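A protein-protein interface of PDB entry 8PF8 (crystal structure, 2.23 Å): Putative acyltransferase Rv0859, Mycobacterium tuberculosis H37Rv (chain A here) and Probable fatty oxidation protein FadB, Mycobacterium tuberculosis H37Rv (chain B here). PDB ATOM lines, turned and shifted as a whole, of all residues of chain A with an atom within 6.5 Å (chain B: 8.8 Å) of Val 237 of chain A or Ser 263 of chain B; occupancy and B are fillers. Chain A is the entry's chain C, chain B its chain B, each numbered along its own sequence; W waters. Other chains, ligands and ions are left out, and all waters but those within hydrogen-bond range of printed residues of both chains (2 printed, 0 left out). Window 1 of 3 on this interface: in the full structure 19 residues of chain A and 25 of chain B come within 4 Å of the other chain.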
ATOM      1  N   ASN A 141      -4.882 -12.831  -2.131  1.00  0.00           N
ATOM      2  CA  ASN A 141      -3.919 -13.828  -1.673  1.00  0.00           C
ATOM      3  C   ASN A 141      -3.730 -13.734  -0.163  1.00  0.00           C
ATOM      4  O   ASN A 141      -3.738 -14.751   0.541  1.00  0.00           O
ATOM      5  CB  ASN A 141      -2.588 -13.635  -2.409  1.00  0.00           C
ATOM      6  CG  ASN A 141      -1.558 -14.715  -2.086  1.00  0.00           C
ATOM      7  OD1 ASN A 141      -1.358 -15.088  -0.931  1.00  0.00           O
ATOM      8  ND2 ASN A 141      -0.885 -15.207  -3.120  1.00  0.00           N
ATOM      9  N   TYR A 142      -3.577 -12.511   0.349  1.00  0.00           N
ATOM     10  CA  TYR A 142      -3.372 -12.308   1.780  1.00  0.00           C
ATOM     11  C   TYR A 142      -4.571 -12.791   2.586  1.00  0.00           C
ATOM     12  O   TYR A 142      -4.411 -13.335   3.686  1.00  0.00           O
ATOM     13  CB  TYR A 142      -3.103 -10.826   2.050  1.00  0.00           C
ATOM     14  CG  TYR A 142      -2.664 -10.480   3.455  1.00  0.00           C
ATOM     15  CD1 TYR A 142      -3.593 -10.165   4.439  1.00  0.00           C
ATOM     16  CD2 TYR A 142      -1.316 -10.437   3.789  1.00  0.00           C
ATOM     17  CE1 TYR A 142      -3.191  -9.833   5.723  1.00  0.00           C
ATOM     18  CE2 TYR A 142      -0.906 -10.109   5.070  1.00  0.00           C
ATOM     19  CZ  TYR A 142      -1.846  -9.809   6.032  1.00  0.00           C
ATOM     20  OH  TYR A 142      -1.436  -9.480   7.304  1.00  0.00           O
ATOM     21  N   MET A 145      -5.280 -16.821   2.443  1.00  0.00           N
ATOM     22  CA  MET A 145      -4.144 -17.558   2.999  1.00  0.00           C
ATOM     23  C   MET A 145      -3.698 -18.668   2.041  1.00  0.00           C
ATOM     24  O   MET A 145      -3.853 -19.865   2.292  1.00  0.00           O
ATOM     25  CB  MET A 145      -4.476 -18.117   4.389  1.00  0.00           C
ATOM     26  CG  MET A 145      -5.097 -17.099   5.341  1.00  0.00           C
ATOM     27  SD  MET A 145      -5.149 -17.682   7.049  1.00  0.00           S
ATOM     28  CE  MET A 145      -6.675 -16.938   7.621  1.00  0.00           C
ATOM     29  N   PHE A 146      -3.135 -18.220   0.921  1.00  0.00           N
ATOM     30  CA  PHE A 146      -2.634 -19.130  -0.102  1.00  0.00           C
ATOM     31  C   PHE A 146      -1.435 -19.905   0.427  1.00  0.00           C
ATOM     32  O   PHE A 146      -0.423 -19.312   0.818  1.00  0.00           O
ATOM     33  CB  PHE A 146      -2.264 -18.347  -1.360  1.00  0.00           C
ATOM     34  CG  PHE A 146      -1.438 -19.127  -2.350  1.00  0.00           C
ATOM     35  CD1 PHE A 146      -2.035 -20.030  -3.215  1.00  0.00           C
ATOM     36  CD2 PHE A 146      -0.066 -18.939  -2.428  1.00  0.00           C
ATOM     37  CE1 PHE A 146      -1.277 -20.741  -4.130  1.00  0.00           C
ATOM     38  CE2 PHE A 146       0.697 -19.648  -3.340  1.00  0.00           C
ATOM     39  CZ  PHE A 146       0.091 -20.549  -4.192  1.00  0.00           C
ATOM     40  N   VAL A 147      -1.552 -21.228   0.444  1.00  0.00           N
ATOM     41  CA  VAL A 147      -0.456 -22.125   0.806  1.00  0.00           C
ATOM     42  C   VAL A 147      -0.368 -23.205  -0.266  1.00  0.00           C
ATOM     43  O   VAL A 147      -1.391 -23.817  -0.601  1.00  0.00           O
ATOM     44  CB  VAL A 147      -0.665 -22.730   2.203  1.00  0.00           C
ATOM     45  CG1 VAL A 147       0.260 -23.911   2.415  1.00  0.00           C
ATOM     46  CG2 VAL A 147      -0.435 -21.679   3.278  1.00  0.00           C
ATOM     47  N   LEU A 231      11.405 -20.026   2.031  1.00  0.00           N
ATOM     48  CA  LEU A 231      11.516 -18.873   1.138  1.00  0.00           C
ATOM     49  C   LEU A 231      10.203 -18.105   1.027  1.00  0.00           C
ATOM     50  O   LEU A 231      10.214 -16.890   0.801  1.00  0.00           O
ATOM     51  CB  LEU A 231      11.971 -19.326  -0.251  1.00  0.00           C
ATOM     52  CG  LEU A 231      13.356 -19.963  -0.366  1.00  0.00           C
ATOM     53  CD1 LEU A 231      13.559 -20.532  -1.763  1.00  0.00           C
ATOM     54  CD2 LEU A 231      14.444 -18.957  -0.029  1.00  0.00           C
ATOM     55  N   GLY A 232       9.068 -18.783   1.182  1.00  0.00           N
ATOM     56  CA  GLY A 232       7.785 -18.119   1.059  1.00  0.00           C
ATOM     57  C   GLY A 232       7.082 -17.873   2.379  1.00  0.00           C
ATOM     58  O   GLY A 232       6.099 -17.128   2.435  1.00  0.00           O
ATOM     59  N   GLY A 233       7.576 -18.488   3.452  1.00  0.00           N
ATOM     60  CA  GLY A 233       6.897 -18.410   4.730  1.00  0.00           C
ATOM     61  C   GLY A 233       5.554 -19.105   4.774  1.00  0.00           C
ATOM     62  O   GLY A 233       4.709 -18.743   5.597  1.00  0.00           O
ATOM     63  N   PHE A 234       5.335 -20.104   3.913  1.00  0.00           N
ATOM     64  CA  PHE A 234       4.031 -20.756   3.838  1.00  0.00           C
ATOM     65  C   PHE A 234       3.762 -21.643   5.049  1.00  0.00           C
ATOM     66  O   PHE A 234       2.597 -21.889   5.383  1.00  0.00           O
ATOM     67  CB  PHE A 234       3.926 -21.570   2.547  1.00  0.00           C
ATOM     68  CG  PHE A 234       4.034 -20.741   1.297  1.00  0.00           C
ATOM     69  CD1 PHE A 234       3.013 -19.877   0.935  1.00  0.00           C
ATOM     70  CD2 PHE A 234       5.150 -20.831   0.480  1.00  0.00           C
ATOM     71  CE1 PHE A 234       3.104 -19.115  -0.216  1.00  0.00           C
ATOM     72  CE2 PHE A 234       5.247 -20.069  -0.673  1.00  0.00           C
ATOM     73  CZ  PHE A 234       4.222 -19.210  -1.019  1.00  0.00           C
ATOM     74  N   ASP A 235       4.813 -22.140   5.707  1.00  0.00           N
ATOM     75  CA  ASP A 235       4.620 -22.894   6.942  1.00  0.00           C
ATOM     76  C   ASP A 235       3.920 -22.044   7.994  1.00  0.00           C
ATOM     77  O   ASP A 235       2.966 -22.492   8.639  1.00  0.00           O
ATOM     78  CB  ASP A 235       5.962 -23.400   7.474  1.00  0.00           C
ATOM     79  CG  ASP A 235       6.270 -24.815   7.029  1.00  0.00           C
ATOM     80  OD1 ASP A 235       5.591 -25.309   6.106  1.00  0.00           O
ATOM     81  OD2 ASP A 235       7.187 -25.437   7.610  1.00  0.00           O
ATOM     82  N   ASP A 236       4.382 -20.804   8.173  1.00  0.00           N
ATOM     83  CA  ASP A 236       3.774 -19.922   9.163  1.00  0.00           C
ATOM     84  C   ASP A 236       2.332 -19.594   8.800  1.00  0.00           C
ATOM     85  O   ASP A 236       1.462 -19.544   9.676  1.00  0.00           O
ATOM     86  CB  ASP A 236       4.600 -18.644   9.301  1.00  0.00           C
ATOM     87  CG  ASP A 236       5.987 -18.905   9.857  1.00  0.00           C
ATOM     88  OD1 ASP A 236       6.649 -19.853   9.385  1.00  0.00           O
ATOM     89  OD2 ASP A 236       6.417 -18.157  10.759  1.00  0.00           O
ATOM     90  N   VAL A 237       2.059 -19.370   7.513  1.00  0.00           N
ATOM     91  CA  VAL A 237       0.692 -19.082   7.086  1.00  0.00           C
ATOM     92  C   VAL A 237      -0.219 -20.269   7.377  1.00  0.00           C
ATOM     93  O   VAL A 237      -1.351 -20.101   7.849  1.00  0.00           O
ATOM     94  CB  VAL A 237       0.667 -18.698   5.593  1.00  0.00           C
ATOM     95  CG1 VAL A 237      -0.763 -18.482   5.119  1.00  0.00           C
ATOM     96  CG2 VAL A 237       1.505 -17.452   5.353  1.00  0.00           C
ATOM     97  N   ALA A 238       0.265 -21.486   7.115  1.00  0.00           N
ATOM     98  CA  ALA A 238      -0.557 -22.672   7.338  1.00  0.00           C
ATOM     99  C   ALA A 238      -0.869 -22.860   8.817  1.00  0.00           C
ATOM    100  O   ALA A 238      -2.011 -23.167   9.183  1.00  0.00           O
ATOM    101  CB  ALA A 238       0.144 -23.907   6.772  1.00  0.00           C
ATOM    102  N   LEU A 239       0.129 -22.673   9.682  1.00  0.00           N
ATOM    103  CA  LEU A 239      -0.075 -22.853  11.114  1.00  0.00           C
ATOM    104  C   LEU A 239      -0.888 -21.729  11.744  1.00  0.00           C
ATOM    105  O   LEU A 239      -1.401 -21.908  12.852  1.00  0.00           O
ATOM    106  CB  LEU A 239       1.276 -22.984  11.821  1.00  0.00           C
ATOM    107  CG  LEU A 239       2.093 -24.215  11.415  1.00  0.00           C
ATOM    108  CD1 LEU A 239       3.349 -24.340  12.260  1.00  0.00           C
ATOM    109  CD2 LEU A 239       1.252 -25.480  11.508  1.00  0.00           C
ATOM    110  N   GLN A 240      -1.025 -20.579  11.075  1.00  0.00           N
ATOM    111  CA  GLN A 240      -1.901 -19.538  11.605  1.00  0.00           C
ATOM    112  C   GLN A 240      -3.362 -19.966  11.564  1.00  0.00           C
ATOM    113  O   GLN A 240      -4.149 -19.558  12.425  1.00  0.00           O
ATOM    114  CB  GLN A 240      -1.706 -18.230  10.835  1.00  0.00           C
ATOM    115  CG  GLN A 240      -0.411 -17.507  11.168  1.00  0.00           C
ATOM    116  CD  GLN A 240      -0.205 -16.245  10.348  1.00  0.00           C
ATOM    117  OE1 GLN A 240      -1.121 -15.758   9.682  1.00  0.00           O
ATOM    118  NE2 GLN A 240       1.007 -15.708  10.392  1.00  0.00           N
ATOM    119  N   LYS A 241      -3.742 -20.780  10.577  1.00  0.00           N
ATOM    120  CA  LYS A 241      -5.087 -21.343  10.523  1.00  0.00           C
ATOM    121  C   LYS A 241      -5.193 -22.619  11.350  1.00  0.00           C
ATOM    122  O   LYS A 241      -6.128 -22.775  12.140  1.00  0.00           O
ATOM    123  CB  LYS A 241      -5.495 -21.622   9.074  1.00  0.00           C
ATOM    124  CG  LYS A 241      -6.922 -22.136   8.945  1.00  0.00           C
ATOM    125  CD  LYS A 241      -7.526 -21.803   7.593  1.00  0.00           C
ATOM    126  CE  LYS A 241      -9.046 -21.878   7.643  1.00  0.00           C
ATOM    127  NZ  LYS A 241      -9.670 -21.403   6.375  1.00  0.00           N
ATOM    128  N   TYR A 242      -4.242 -23.537  11.179  1.00  0.00           N
ATOM    129  CA  TYR A 242      -4.192 -24.767  11.972  1.00  0.00           C
ATOM    130  C   TYR A 242      -3.328 -24.525  13.211  1.00  0.00           C
ATOM    131  O   TYR A 242      -2.236 -25.070  13.378  1.00  0.00           O
ATOM    132  CB  TYR A 242      -3.677 -25.922  11.122  1.00  0.00           C
ATOM    133  CG  TYR A 242      -4.636 -26.304  10.015  1.00  0.00           C
ATOM    134  CD1 TYR A 242      -4.616 -25.650   8.789  1.00  0.00           C
ATOM    135  CD2 TYR A 242      -5.577 -27.305  10.207  1.00  0.00           C
ATOM    136  CE1 TYR A 242      -5.502 -25.991   7.782  1.00  0.00           C
ATOM    137  CE2 TYR A 242      -6.465 -27.653   9.209  1.00  0.00           C
ATOM    138  CZ  TYR A 242      -6.426 -26.994   8.000  1.00  0.00           C
ATOM    139  OH  TYR A 242      -7.315 -27.349   7.012  1.00  0.00           O
ATOM    140  N   VAL A 297      -6.543 -24.264   2.576  1.00  0.00           N
ATOM    141  CA  VAL A 297      -5.154 -24.181   3.018  1.00  0.00           C
ATOM    142  C   VAL A 297      -4.516 -25.564   3.075  1.00  0.00           C
ATOM    143  O   VAL A 297      -3.383 -25.750   2.623  1.00  0.00           O
ATOM    144  CB  VAL A 297      -5.062 -23.457   4.380  1.00  0.00           C
ATOM    145  CG1 VAL A 297      -3.605 -23.239   4.764  1.00  0.00           C
ATOM    146  CG2 VAL A 297      -5.809 -22.130   4.330  1.00  0.00           C
ATOM    147  N   ILE B 257       8.073 -15.500  -8.067  1.00  0.00           N
ATOM    148  CA  ILE B 257       8.164 -15.256  -6.628  1.00  0.00           C
ATOM    149  C   ILE B 257       7.023 -14.397  -6.098  1.00  0.00           C
ATOM    150  O   ILE B 257       6.818 -14.352  -4.874  1.00  0.00           O
ATOM    151  CB  ILE B 257       9.513 -14.601  -6.262  1.00  0.00           C
ATOM    152  CG1 ILE B 257       9.568 -13.159  -6.766  1.00  0.00           C
ATOM    153  CG2 ILE B 257      10.668 -15.386  -6.852  1.00  0.00           C
ATOM    154  CD1 ILE B 257      10.849 -12.436  -6.387  1.00  0.00           C
ATOM    155  N   LEU B 258       6.279 -13.718  -6.972  1.00  0.00           N
ATOM    156  CA  LEU B 258       5.253 -12.782  -6.515  1.00  0.00           C
ATOM    157  C   LEU B 258       4.182 -13.409  -5.626  1.00  0.00           C
ATOM    158  O   LEU B 258       3.707 -12.714  -4.710  1.00  0.00           O
ATOM    159  CB  LEU B 258       4.610 -12.098  -7.731  1.00  0.00           C
ATOM    160  CG  LEU B 258       3.805 -10.824  -7.475  1.00  0.00           C
ATOM    161  CD1 LEU B 258       4.648  -9.805  -6.734  1.00  0.00           C
ATOM    162  CD2 LEU B 258       3.324 -10.247  -8.792  1.00  0.00           C
ATOM    163  N   PRO B 259       3.741 -14.657  -5.830  1.00  0.00           N
ATOM    164  CA  PRO B 259       2.791 -15.251  -4.874  1.00  0.00           C
ATOM    165  C   PRO B 259       3.324 -15.367  -3.455  1.00  0.00           C
ATOM    166  O   PRO B 259       2.521 -15.475  -2.520  1.00  0.00           O
ATOM    167  CB  PRO B 259       2.512 -16.636  -5.475  1.00  0.00           C
ATOM    168  CG  PRO B 259       2.724 -16.450  -6.924  1.00  0.00           C
ATOM    169  CD  PRO B 259       3.864 -15.485  -7.046  1.00  0.00           C
ATOM    170  N   SER B 260       4.643 -15.351  -3.258  1.00  0.00           N
ATOM    171  CA  SER B 260       5.207 -15.482  -1.921  1.00  0.00           C
ATOM    172  C   SER B 260       5.243 -14.168  -1.151  1.00  0.00           C
ATOM    173  O   SER B 260       5.525 -14.187   0.053  1.00  0.00           O
ATOM    174  CB  SER B 260       6.625 -16.057  -1.998  1.00  0.00           C
ATOM    175  OG  SER B 260       7.526 -15.116  -2.557  1.00  0.00           O
ATOM    176  N   PHE B 261       4.970 -13.032  -1.806  1.00  0.00           N
ATOM    177  CA  PHE B 261       5.058 -11.752  -1.102  1.00  0.00           C
ATOM    178  C   PHE B 261       3.977 -11.609  -0.036  1.00  0.00           C
ATOM    179  O   PHE B 261       4.305 -11.196   1.090  1.00  0.00           O
ATOM    180  CB  PHE B 261       5.024 -10.588  -2.102  1.00  0.00           C
ATOM    181  CG  PHE B 261       6.259 -10.469  -2.963  1.00  0.00           C
ATOM    182  CD1 PHE B 261       7.251 -11.438  -2.940  1.00  0.00           C
ATOM    183  CD2 PHE B 261       6.428  -9.372  -3.793  1.00  0.00           C
ATOM    184  CE1 PHE B 261       8.378 -11.321  -3.736  1.00  0.00           C
ATOM    185  CE2 PHE B 261       7.552  -9.248  -4.588  1.00  0.00           C
ATOM    186  CZ  PHE B 261       8.529 -10.223  -4.558  1.00  0.00           C
ATOM    187  N   PRO B 262       2.698 -11.911  -0.298  1.00  0.00           N
ATOM    188  CA  PRO B 262       1.709 -11.826   0.791  1.00  0.00           C
ATOM    189  C   PRO B 262       1.961 -12.812   1.919  1.00  0.00           C
ATOM    190  O   PRO B 262       1.675 -12.491   3.080  1.00  0.00           O
ATOM    191  CB  PRO B 262       0.377 -12.112   0.082  1.00  0.00           C
ATOM    192  CG  PRO B 262       0.629 -11.796  -1.348  1.00  0.00           C
ATOM    193  CD  PRO B 262       2.047 -12.196  -1.590  1.00  0.00           C
ATOM    194  N   SER B 263       2.486 -14.004   1.619  1.00  0.00           N
ATOM    195  CA  SER B 263       2.725 -14.989   2.671  1.00  0.00           C
ATOM    196  C   SER B 263       3.914 -14.602   3.544  1.00  0.00           C
ATOM    197  O   SER B 263       3.900 -14.843   4.757  1.00  0.00           O
ATOM    198  CB  SER B 263       2.932 -16.375   2.059  1.00  0.00           C
ATOM    199  OG  SER B 263       3.988 -16.363   1.115  1.00  0.00           O
ATOM    200  N   ASN B 264       4.954 -14.008   2.951  1.00  0.00           N
ATOM    201  CA  ASN B 264       6.071 -13.517   3.753  1.00  0.00           C
ATOM    202  C   ASN B 264       5.641 -12.351   4.633  1.00  0.00           C
ATOM    203  O   ASN B 264       6.104 -12.221   5.772  1.00  0.00           O
ATOM    204  CB  ASN B 264       7.234 -13.106   2.849  1.00  0.00           C
ATOM    205  CG  ASN B 264       8.153 -14.267   2.513  1.00  0.00           C
ATOM    206  OD1 ASN B 264       8.566 -15.024   3.392  1.00  0.00           O
ATOM    207  ND2 ASN B 264       8.476 -14.411   1.233  1.00  0.00           N
ATOM    208  N   LEU B 265       4.760 -11.491   4.118  1.00  0.00           N
ATOM    209  CA  LEU B 265       4.237 -10.392   4.922  1.00  0.00           C
ATOM    210  C   LEU B 265       3.411 -10.918   6.087  1.00  0.00           C
ATOM    211  O   LEU B 265       3.504 -10.406   7.210  1.00  0.00           O
ATOM    212  CB  LEU B 265       3.403  -9.455   4.046  1.00  0.00           C
ATOM    213  CG  LEU B 265       2.737  -8.256   4.726  1.00  0.00           C
ATOM    214  CD1 LEU B 265       3.777  -7.291   5.273  1.00  0.00           C
ATOM    215  CD2 LEU B 265       1.802  -7.548   3.764  1.00  0.00           C
ATOM    216  N   ARG B 266       2.603 -11.949   5.841  1.00  0.00           N
ATOM    217  CA  ARG B 266       1.817 -12.554   6.908  1.00  0.00           C
ATOM    218  C   ARG B 266       2.708 -13.241   7.936  1.00  0.00           C
ATOM    219  O   ARG B 266       2.357 -13.299   9.121  1.00  0.00           O
ATOM    220  CB  ARG B 266       0.814 -13.541   6.310  1.00  0.00           C
ATOM    221  CG  ARG B 266      -0.449 -13.714   7.122  1.00  0.00           C
ATOM    222  CD  ARG B 266      -1.475 -14.532   6.362  1.00  0.00           C
ATOM    223  NE  ARG B 266      -2.687 -14.734   7.146  1.00  0.00           N
ATOM    224  CZ  ARG B 266      -3.742 -13.932   7.109  1.00  0.00           C
ATOM    225  NH1 ARG B 266      -3.772 -12.867   6.328  1.00  0.00           N
ATOM    226  NH2 ARG B 266      -4.793 -14.208   7.875  1.00  0.00           N
ATOM    227  N   LYS B 267       3.861 -13.761   7.506  1.00  0.00           N
ATOM    228  CA  LYS B 267       4.812 -14.343   8.447  1.00  0.00           C
ATOM    229  C   LYS B 267       5.437 -13.274   9.336  1.00  0.00           C
ATOM    230  O   LYS B 267       5.575 -13.470  10.549  1.00  0.00           O
ATOM    231  CB  LYS B 267       5.893 -15.114   7.686  1.00  0.00           C
ATOM    232  CG  LYS B 267       7.164 -15.364   8.483  1.00  0.00           C
ATOM    233  CD  LYS B 267       8.158 -16.205   7.699  1.00  0.00           C
ATOM    234  CE  LYS B 267       9.465 -16.352   8.458  1.00  0.00           C
ATOM    235  NZ  LYS B 267      10.399 -17.292   7.780  1.00  0.00           N
ATOM    236  N   GLN B 268       5.816 -12.134   8.751  1.00  0.00           N
ATOM    237  CA  GLN B 268       6.431 -11.067   9.535  1.00  0.00           C
ATOM    238  C   GLN B 268       5.443 -10.462  10.525  1.00  0.00           C
ATOM    239  O   GLN B 268       5.806 -10.171  11.671  1.00  0.00           O
ATOM    240  CB  GLN B 268       6.987  -9.990   8.604  1.00  0.00           C
ATOM    241  CG  GLN B 268       8.178 -10.448   7.784  1.00  0.00           C
ATOM    242  CD  GLN B 268       9.396 -10.719   8.641  1.00  0.00           C
ATOM    243  OE1 GLN B 268       9.790  -9.889   9.461  1.00  0.00           O
ATOM    244  NE2 GLN B 268       9.997 -11.893   8.463  1.00  0.00           N
ATOM    245  N   LEU B 269       4.194 -10.260  10.101  1.00  0.00           N
ATOM    246  CA  LEU B 269       3.156  -9.749  10.988  1.00  0.00           C
ATOM    247  C   LEU B 269       2.615 -10.806  11.941  1.00  0.00           C
ATOM    248  O   LEU B 269       1.874 -10.456  12.866  1.00  0.00           O
ATOM    249  CB  LEU B 269       1.999  -9.169  10.171  1.00  0.00           C
ATOM    250  CG  LEU B 269       2.319  -7.966   9.283  1.00  0.00           C
ATOM    251  CD1 LEU B 269       1.067  -7.504   8.555  1.00  0.00           C
ATOM    252  CD2 LEU B 269       2.919  -6.832  10.101  1.00  0.00           C
ATOM    253  N   LYS B 270       2.959 -12.080  11.730  1.00  0.00           N
ATOM    254  CA  LYS B 270       2.528 -13.187  12.585  1.00  0.00           C
ATOM    255  C   LYS B 270       1.006 -13.291  12.658  1.00  0.00           C
ATOM    256  O   LYS B 270       0.450 -13.748  13.661  1.00  0.00           O
ATOM    257  CB  LYS B 270       3.135 -13.071  13.989  1.00  0.00           C
ATOM    258  CG  LYS B 270       4.638 -12.818  13.978  1.00  0.00           C
ATOM    259  CD  LYS B 270       5.383 -13.707  14.964  1.00  0.00           C
ATOM    260  CE  LYS B 270       5.460 -13.076  16.344  1.00  0.00           C
ATOM    261  NZ  LYS B 270       6.263 -11.820  16.347  1.00  0.00           N
ATOM    262  N   GLY B 271       0.321 -12.880  11.594  1.00  0.00           N
ATOM    263  CA  GLY B 271      -1.124 -12.938  11.548  1.00  0.00           C
ATOM    264  C   GLY B 271      -1.841 -11.803  12.242  1.00  0.00           C
ATOM    265  O   GLY B 271      -3.069 -11.862  12.380  1.00  0.00           O
ATOM    266  N   LEU B 281       1.116  -3.307  -0.050  1.00  0.00           N
ATOM    267  CA  LEU B 281       1.539  -4.337  -0.994  1.00  0.00           C
ATOM    268  C   LEU B 281       0.561  -4.451  -2.154  1.00  0.00           C
ATOM    269  O   LEU B 281       0.972  -4.594  -3.312  1.00  0.00           O
ATOM    270  CB  LEU B 281       1.684  -5.680  -0.278  1.00  0.00           C
ATOM    271  CG  LEU B 281       2.154  -6.872  -1.119  1.00  0.00           C
ATOM    272  CD1 LEU B 281       3.506  -6.588  -1.757  1.00  0.00           C
ATOM    273  CD2 LEU B 281       2.216  -8.133  -0.274  1.00  0.00           C
ATOM    274  N   GLN B 553      -0.181 -19.173  19.318  1.00  0.00           N
ATOM    275  CA  GLN B 553      -0.700 -18.548  18.106  1.00  0.00           C
ATOM    276  C   GLN B 553      -1.651 -17.407  18.443  1.00  0.00           C
ATOM    277  O   GLN B 553      -1.675 -16.386  17.746  1.00  0.00           O
ATOM    278  CB  GLN B 553      -1.400 -19.586  17.228  1.00  0.00           C
ATOM    279  CG  GLN B 553      -0.456 -20.470  16.427  1.00  0.00           C
ATOM    280  CD  GLN B 553       0.129 -19.760  15.219  1.00  0.00           C
ATOM    281  OE1 GLN B 553      -0.207 -18.609  14.935  1.00  0.00           O
ATOM    282  NE2 GLN B 553       1.005 -20.449  14.497  1.00  0.00           N
ATOM    283  N   GLN B 557      -0.965 -13.763  16.966  1.00  0.00           N
ATOM    284  CA  GLN B 557      -1.983 -13.200  16.086  1.00  0.00           C
ATOM    285  C   GLN B 557      -2.745 -12.057  16.743  1.00  0.00           C
ATOM    286  O   GLN B 557      -3.375 -11.261  16.036  1.00  0.00           O
ATOM    287  CB  GLN B 557      -2.946 -14.294  15.627  1.00  0.00           C
ATOM    288  CG  GLN B 557      -2.276 -15.373  14.791  1.00  0.00           C
ATOM    289  CD  GLN B 557      -3.255 -16.384  14.237  1.00  0.00           C
ATOM    290  OE1 GLN B 557      -4.325 -16.026  13.746  1.00  0.00           O
ATOM    291  NE2 GLN B 557      -2.893 -17.661  14.312  1.00  0.00           N
HETATM  292  O   HOH W   1       5.321 -15.912  12.188  1.00  0.00           O
HETATM  293  O   HOH W   2       2.466 -19.564  12.210  1.00  0.00           O
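Of chain B, only Ser 263 comes within 4 Å of Val 237 of chain A. Of chain A, only Gly 232 (2.6 Å), Phe 234 (3.2 Å) and Val 237 (3.6 Å) come within 4 Å of Ser 263 of chain B. Of the printed residues of chain A, Pro 262 of chain B touches Asn 141 and Tyr 142. Of the printed residues of chain B, Asn 141 of chain A touches Pro 259 (3.5 Å) and Pro 262 (3.6 Å). Printed residues of chain A within 4 Å of Leu 269 of chain B: Tyr 142. Of the printed residues of chain A, Arg 266 of chain B touches Tyr 142, Met 145 and Gln 240.
Among the printed residues, pairs that only touch across the chains: Asn 141 of chain A with Pro 262 of chain B (3.6 Å), Tyr 142 of chain A with Pro 262 of chain B (3.7 Å), Tyr 142 of chain A with Leu 265 of chain B (3.9 Å), Tyr 142 of chain A with Leu 269 of chain B (3.4 Å), Gly 232 of chain A with Ser 260 of chain B (3.8 Å), Gly 233 of chain A with Asn 264 of chain B (3.6 Å), Gly 233 of chain A with Lys 267 of chain B (3.9 Å), Phe 234 of chain A with Ser 260 of chain B (3.96 Å), Phe 234 of chain A with Ser 263 of chain B (3.2 Å), Asp 236 of chain A with Lys 267 of chain B (3.7 Å), Val 237 of chain A with Ser 263 of chain B (3.6 Å), Gln 240 of chain A with Lys 270 of chain B (3.3 Å) and Gln 240 of chain A with Gln 553 of chain B (3.8 Å).
Printed residues of chain B that touch a printed residue of chain A: Pro 259, Ser 260, Pro 262, Ser 263, Asn 264, Leu 265, Arg 266, Lys 267, Leu 269, Lys 270, Gly 271, Gln 553 and Gln 557. Hydrophobic or aromatic side chains of chain B within 4 Å of the printed part of chain A: Pro 262, Leu 265 and Leu 269. Of the 18 printed residues of chain A, 11 touch a printed residue of chain B. Hydrophobic or aromatic side chains of chain A within 4 Å of the printed part of chain B: Tyr 142, Met 145, Phe 234, Val 237 and Leu 239. Among the printed residues, no Asp or Glu carboxylate lies within 4 Å of a Lys or Arg side-chain nitrogen of the other chain.
Water W2 lies within hydrogen-bond range of the backbone carbonyl oxygen (O) of Asp 236 of chain A (2.7 Å) and the side-chain amide nitrogen (NE2) of Gln 553 of chain B (2.9 Å). Water W1 lies within hydrogen-bond range of the side-chain carboxylate of Asp 236 of chain A (2.9 Å) and the backbone carbonyl oxygen of Lys 267 of chain B (3.0 Å).
OG of Ser 260 of chain B is in hydrogen-bond range of O of Ile 257 of chain B (2.5 Å). O of Ser 260 of chain B sits at hydrogen-bond distance from OG of Ser 263 of chain B (2.9 Å). The side-chain amide nitrogen (ND2) of Asn 264 of chain B is in hydrogen-bond range of the backbone carbonyl oxygen (O) of Ser 260 of chain B (3.2 Å). O of Arg 266 of chain B is in hydrogen-bond range of N of Gly 271 of chain B (3.2 Å). OE1 of Gln 553 of chain B lies within hydrogen-bond range of NE2 of Gln 557 of chain B (2.9 Å).
The backbone carbonyl oxygen (O) of Pro 259 of chain B lies within hydrogen-bond range of the side-chain amide nitrogen (ND2) of Asn 141 of chain A, 3.5 Å away. The backbone carbonyl oxygen (O) of Gly 232 of chain A is in hydrogen-bond range of the side-chain hydroxyl (OG) of Ser 263 of chain B, at 2.6 Å. The side-chain amide nitrogen (ND2) of Asn 264 of chain B lies within hydrogen-bond range of the backbone carbonyl oxygen (O) of Leu 231 of chain A (3.1 Å). The backbone NH (N) of Asn 264 of chain B sits at hydrogen-bond distance from the backbone carbonyl oxygen (O) of Gly 232 of chain A (3.4 Å). The guanidinium group (NH1) of Arg 266 of chain B lies within hydrogen-bond range of the backbone carbonyl oxygen (O) of Tyr 142 of chain A, 2.8 Å away. The side-chain sulfur (SD) of Met 145 of chain A lies close to the guanidinium group (NH2) of Arg 266 of chain B, at 3.6 Å. O of Arg 266 of chain B sits at hydrogen-bond distance from NE2 of Gln 240 of chain A. The backbone NH of Gly 271 of chain B sits close to the side-chain amide nitrogen of Gln 240 of chain A (3.1 Å). NE2 of Gln 553 of chain B is in hydrogen-bond range of O of Leu 239 of chain A, 3.3 Å away. The side-chain amide nitrogen of Gln 557 of chain B is in hydrogen-bond range of the backbone carbonyl oxygen of Gln 240 of chain A (3.0 Å).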
